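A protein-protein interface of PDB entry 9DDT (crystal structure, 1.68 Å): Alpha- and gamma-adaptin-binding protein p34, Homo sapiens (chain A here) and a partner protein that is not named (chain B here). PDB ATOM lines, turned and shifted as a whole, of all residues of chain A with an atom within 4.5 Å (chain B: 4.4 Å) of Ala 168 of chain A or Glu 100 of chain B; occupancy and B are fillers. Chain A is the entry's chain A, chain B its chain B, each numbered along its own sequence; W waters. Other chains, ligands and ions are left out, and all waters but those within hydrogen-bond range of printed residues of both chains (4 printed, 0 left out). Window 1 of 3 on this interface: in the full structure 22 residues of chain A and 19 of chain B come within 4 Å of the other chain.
Water W4 bridges the side-chain carboxylate (OE2) of Glu 100 of chain B and the guanidinium group (NH2) of Arg 161 of chain A. Water W2 lies within hydrogen-bond range of NH1 of Arg 161 of chain A and OE2 of Glu 100 of chain B. Water W1 lies within hydrogen-bond range of the guanidinium group of Arg 15 of chain B (2.8 Å), the backbone carbonyl oxygen of Ala 168 of chain A (2.9 Å) and the side-chain amide oxygen of Asn 169 of chain A (2.9 Å). Water W3 bridges NH2 of Arg 161 of chain A and OG of Ser 9 of chain B.
NE of Arg 15 of chain B lies within salt-bridge range of OE1 of Glu 100 of chain B (2.8 Å).
Leu 101 of chain B touches Asn 167 of chain A. O of Ala 168 of chain A touches NH2 of Arg 15 of chain B, 3.9 Å away. Ala 168 of chain A touches Glu 100 of chain B (CB to OE2, 3.95 Å). CD1 of Leu 101 of chain B touches CA of Ala 168 of chain A (3.9 Å). Ala 168 of chain A touches Ile 104 of chain B (C to CD1, 3.7 Å).
Of the 9 printed residues of chain B, 4 touch a printed residue of chain A. Printed residues of chain B that touch a printed residue of chain A: Arg 15, Glu 100, Leu 101 and Ile 104. Printed residues of chain A that touch a printed residue of chain B: Asn 167 and Ala 168.
Ala 168 of chain A touches four residues of chain B. Of the printed residues of chain A, Arg 15 of chain B touches Ala 168 (3.9 Å). Of chain A, only Ala 168 comes within 4 Å of Glu 100 of chain B. Of the printed residues of chain A, Leu 101 of chain B touches Asn 167 (3.2 Å) and Ala 168 (3.9 Å). The nearest printed residue of chain A that does not touch Ile 104 of chain B is Asn 169 of chain A (4.2 Å).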
ATOM      1  N   VAL A 109     -13.209   9.243   7.412  1.00  0.00           N
ATOM      2  CA  VAL A 109     -13.599   7.871   7.693  1.00  0.00           C
ATOM      3  C   VAL A 109     -14.950   7.621   7.033  1.00  0.00           C
ATOM      4  O   VAL A 109     -15.927   8.318   7.327  1.00  0.00           O
ATOM      5  CB  VAL A 109     -13.683   7.590   9.201  1.00  0.00           C
ATOM      6  CG1 VAL A 109     -14.154   6.162   9.422  1.00  0.00           C
ATOM      7  CG2 VAL A 109     -12.327   7.840   9.883  1.00  0.00           C
ATOM      8  N   ARG A 161     -14.148  -3.547  14.310  1.00  0.00           N
ATOM      9  CA  ARG A 161     -13.471  -2.876  13.202  1.00  0.00           C
ATOM     10  C   ARG A 161     -13.969  -1.444  13.034  1.00  0.00           C
ATOM     11  O   ARG A 161     -13.181  -0.527  12.758  1.00  0.00           O
ATOM     12  CB  ARG A 161     -13.656  -3.686  11.913  1.00  0.00           C
ATOM     13  CG  ARG A 161     -13.061  -3.034  10.667  1.00  0.00           C
ATOM     14  CD  ARG A 161     -11.565  -2.743  10.819  1.00  0.00           C
ATOM     15  NE  ARG A 161     -11.168  -1.718   9.852  1.00  0.00           N
ATOM     16  CZ  ARG A 161     -10.175  -0.852  10.035  1.00  0.00           C
ATOM     17  NH1 ARG A 161      -9.431  -0.890  11.143  1.00  0.00           N
ATOM     18  NH2 ARG A 161      -9.927   0.059   9.103  1.00  0.00           N
ATOM     19  N   GLN A 164     -12.222   0.558  15.649  1.00  0.00           N
ATOM     20  CA  GLN A 164     -10.831   0.760  15.251  1.00  0.00           C
ATOM     21  C   GLN A 164     -10.716   1.856  14.194  1.00  0.00           C
ATOM     22  O   GLN A 164      -9.858   2.744  14.288  1.00  0.00           O
ATOM     23  CB  GLN A 164     -10.279  -0.552  14.716  1.00  0.00           C
ATOM     24  CG  GLN A 164      -8.824  -0.560  14.410  1.00  0.00           C
ATOM     25  CD  GLN A 164      -8.377  -1.964  14.027  1.00  0.00           C
ATOM     26  OE1 GLN A 164      -9.180  -2.761  13.520  1.00  0.00           O
ATOM     27  NE2 GLN A 164      -7.120  -2.293  14.319  1.00  0.00           N
ATOM     28  N   ALA A 165     -11.595   1.825  13.191  1.00  0.00           N
ATOM     29  CA  ALA A 165     -11.532   2.800  12.110  1.00  0.00           C
ATOM     30  C   ALA A 165     -11.819   4.203  12.618  1.00  0.00           C
ATOM     31  O   ALA A 165     -11.188   5.168  12.174  1.00  0.00           O
ATOM     32  CB  ALA A 165     -12.513   2.417  10.996  1.00  0.00           C
ATOM     33  N   LEU A 166     -12.780   4.338  13.544  1.00  0.00           N
ATOM     34  CA  LEU A 166     -13.082   5.655  14.105  1.00  0.00           C
ATOM     35  C   LEU A 166     -11.942   6.169  14.988  1.00  0.00           C
ATOM     36  O   LEU A 166     -11.755   7.389  15.104  1.00  0.00           O
ATOM     37  CB  LEU A 166     -14.403   5.596  14.891  1.00  0.00           C
ATOM     38  CG  LEU A 166     -15.655   5.375  14.031  1.00  0.00           C
ATOM     39  CD1 LEU A 166     -16.860   5.014  14.909  1.00  0.00           C
ATOM     40  CD2 LEU A 166     -15.966   6.574  13.121  1.00  0.00           C
ATOM     41  N   ASN A 167     -11.184   5.264  15.625  1.00  0.00           N
ATOM     42  CA  ASN A 167      -9.990   5.654  16.375  1.00  0.00           C
ATOM     43  C   ASN A 167      -8.889   6.138  15.435  1.00  0.00           C
ATOM     44  O   ASN A 167      -8.172   7.098  15.744  1.00  0.00           O
ATOM     45  CB  ASN A 167      -9.510   4.463  17.207  1.00  0.00           C
ATOM     46  CG  ASN A 167     -10.126   4.434  18.599  1.00  0.00           C
ATOM     47  OD1 ASN A 167      -9.546   4.937  19.570  1.00  0.00           O
ATOM     48  ND2 ASN A 167     -11.347   3.915  18.688  1.00  0.00           N
ATOM     49  N   ALA A 168      -8.777   5.522  14.257  1.00  0.00           N
ATOM     50  CA  ALA A 168      -7.711   5.846  13.299  1.00  0.00           C
ATOM     51  C   ALA A 168      -8.104   7.070  12.467  1.00  0.00           C
ATOM     52  O   ALA A 168      -8.333   7.009  11.254  1.00  0.00           O
ATOM     53  CB  ALA A 168      -7.429   4.644  12.407  1.00  0.00           C
ATOM     54  N   ASN A 169      -8.200   8.207  13.154  1.00  0.00           N
ATOM     55  CA  ASN A 169      -8.695   9.436  12.553  1.00  0.00           C
ATOM     56  C   ASN A 169      -8.230  10.599  13.411  1.00  0.00           C
ATOM     57  O   ASN A 169      -8.201  10.501  14.646  1.00  0.00           O
ATOM     58  CB  ASN A 169     -10.227   9.450  12.452  1.00  0.00           C
ATOM     59  CG  ASN A 169     -10.735  10.529  11.537  1.00  0.00           C
ATOM     60  OD1 ASN A 169     -10.155  10.799  10.486  1.00  0.00           O
ATOM     61  ND2 ASN A 169     -11.835  11.160  11.926  1.00  0.00           N
ATOM     62  N   SER B   9      -4.369   2.080   3.752  1.00  0.00           N
ATOM     63  CA  SER B   9      -5.498   1.421   4.404  1.00  0.00           C
ATOM     64  C   SER B   9      -6.522   0.894   3.394  1.00  0.00           C
ATOM     65  O   SER B   9      -6.469   1.176   2.191  1.00  0.00           O
ATOM     66  CB  SER B   9      -6.172   2.412   5.367  1.00  0.00           C
ATOM     67  OG  SER B   9      -6.975   3.327   4.627  1.00  0.00           O
ATOM     68  N   ARG B  15      -0.746   6.180   4.302  1.00  0.00           N
ATOM     69  CA  ARG B  15      -0.265   6.551   5.626  1.00  0.00           C
ATOM     70  C   ARG B  15       1.247   6.679   5.689  1.00  0.00           C
ATOM     71  O   ARG B  15       1.762   7.438   6.522  1.00  0.00           O
ATOM     72  CB  ARG B  15      -0.726   5.526   6.671  1.00  0.00           C
ATOM     73  CG  ARG B  15      -2.263   5.493   6.856  1.00  0.00           C
ATOM     74  CD  ARG B  15      -2.816   6.897   7.090  1.00  0.00           C
ATOM     75  NE  ARG B  15      -4.233   6.830   7.436  1.00  0.00           N
ATOM     76  CZ  ARG B  15      -5.007   7.884   7.651  1.00  0.00           C
ATOM     77  NH1 ARG B  15      -4.525   9.113   7.530  1.00  0.00           N
ATOM     78  NH2 ARG B  15      -6.285   7.695   7.966  1.00  0.00           N
ATOM     79  N   LEU B  65      -3.816  -2.891   7.098  1.00  0.00           N
ATOM     80  CA  LEU B  65      -2.845  -2.094   6.360  1.00  0.00           C
ATOM     81  C   LEU B  65      -2.290  -2.928   5.216  1.00  0.00           C
ATOM     82  O   LEU B  65      -2.047  -4.121   5.379  1.00  0.00           O
ATOM     83  CB  LEU B  65      -1.696  -1.648   7.273  1.00  0.00           C
ATOM     84  CG  LEU B  65      -1.928  -0.457   8.201  1.00  0.00           C
ATOM     85  CD1 LEU B  65      -0.693  -0.292   9.105  1.00  0.00           C
ATOM     86  CD2 LEU B  65      -2.175   0.770   7.357  1.00  0.00           C
ATOM     87  N   CYS B  99      -0.788  -1.479  13.697  1.00  0.00           N
ATOM     88  CA  CYS B  99      -2.012  -0.678  13.661  1.00  0.00           C
ATOM     89  C   CYS B  99      -1.821   0.595  12.843  1.00  0.00           C
ATOM     90  O   CYS B  99      -0.816   1.296  12.985  1.00  0.00           O
ATOM     91  CB  CYS B  99      -2.470  -0.276  15.090  1.00  0.00           C
ATOM     92  SG  CYS B  99      -2.944  -1.673  16.142  1.00  0.00           S
ATOM     93  N   GLU B 100      -2.817   0.909  12.008  1.00  0.00           N
ATOM     94  CA  GLU B 100      -2.851   2.196  11.329  1.00  0.00           C
ATOM     95  C   GLU B 100      -2.726   3.357  12.315  1.00  0.00           C
ATOM     96  O   GLU B 100      -2.165   4.410  11.982  1.00  0.00           O
ATOM     97  CB  GLU B 100      -4.154   2.324  10.519  1.00  0.00           C
ATOM     98  CG  GLU B 100      -4.251   3.560   9.613  1.00  0.00           C
ATOM     99  CD  GLU B 100      -5.612   3.675   8.926  1.00  0.00           C
ATOM    100  OE1 GLU B 100      -5.860   4.678   8.227  1.00  0.00           O
ATOM    101  OE2 GLU B 100      -6.430   2.746   9.089  1.00  0.00           O
ATOM    102  N   LEU B 101      -3.294   3.201  13.508  1.00  0.00           N
ATOM    103  CA  LEU B 101      -3.232   4.266  14.500  1.00  0.00           C
ATOM    104  C   LEU B 101      -1.790   4.669  14.788  1.00  0.00           C
ATOM    105  O   LEU B 101      -1.479   5.868  14.913  1.00  0.00           O
ATOM    106  CB  LEU B 101      -3.954   3.812  15.768  1.00  0.00           C
ATOM    107  CG  LEU B 101      -4.196   4.877  16.825  1.00  0.00           C
ATOM    108  CD1 LEU B 101      -5.277   5.830  16.386  1.00  0.00           C
ATOM    109  CD2 LEU B 101      -4.622   4.184  18.129  1.00  0.00           C
ATOM    110  N   ASP B 102      -0.889   3.681  14.880  1.00  0.00           N
ATOM    111  CA  ASP B 102       0.516   3.974  15.141  1.00  0.00           C
ATOM    112  C   ASP B 102       1.153   4.714  13.978  1.00  0.00           C
ATOM    113  O   ASP B 102       1.965   5.619  14.189  1.00  0.00           O
ATOM    114  CB  ASP B 102       1.302   2.688  15.425  1.00  0.00           C
ATOM    115  CG  ASP B 102       0.777   1.933  16.625  1.00  0.00           C
ATOM    116  OD1 ASP B 102       0.660   2.569  17.686  1.00  0.00           O
ATOM    117  OD2 ASP B 102       0.511   0.711  16.527  1.00  0.00           O
ATOM    118  N   ILE B 103       0.814   4.338  12.741  1.00  0.00           N
ATOM    119  CA  ILE B 103       1.408   5.025  11.603  1.00  0.00           C
ATOM    120  C   ILE B 103       0.906   6.456  11.509  1.00  0.00           C
ATOM    121  O   ILE B 103       1.644   7.348  11.075  1.00  0.00           O
ATOM    122  CB  ILE B 103       1.171   4.245  10.296  1.00  0.00           C
ATOM    123  CG1 ILE B 103       1.339   2.743  10.543  1.00  0.00           C
ATOM    124  CG2 ILE B 103       2.110   4.757   9.207  1.00  0.00           C
ATOM    125  CD1 ILE B 103       2.803   2.335  10.879  1.00  0.00           C
ATOM    126  N   ILE B 104      -0.336   6.715  11.933  1.00  0.00           N
ATOM    127  CA  ILE B 104      -0.866   8.078  11.886  1.00  0.00           C
ATOM    128  C   ILE B 104      -0.165   8.963  12.911  1.00  0.00           C
ATOM    129  O   ILE B 104       0.264  10.083  12.595  1.00  0.00           O
ATOM    130  CB  ILE B 104      -2.389   8.079  12.118  1.00  0.00           C
ATOM    131  CG1 ILE B 104      -3.115   7.363  10.971  1.00  0.00           C
ATOM    132  CG2 ILE B 104      -2.884   9.521  12.279  1.00  0.00           C
ATOM    133  CD1 ILE B 104      -4.620   7.156  11.238  1.00  0.00           C
HETATM  134  O   HOH W   1      -8.736   8.705   8.976  1.00  0.00           O
HETATM  135  O   HOH W   2      -7.379   1.014  11.581  1.00  0.00           O
HETATM  136  O   HOH W   3      -9.339   1.638   6.252  1.00  0.00           O
HETATM  137  O   HOH W   4      -8.810   2.674   9.480  1.00  0.00           O
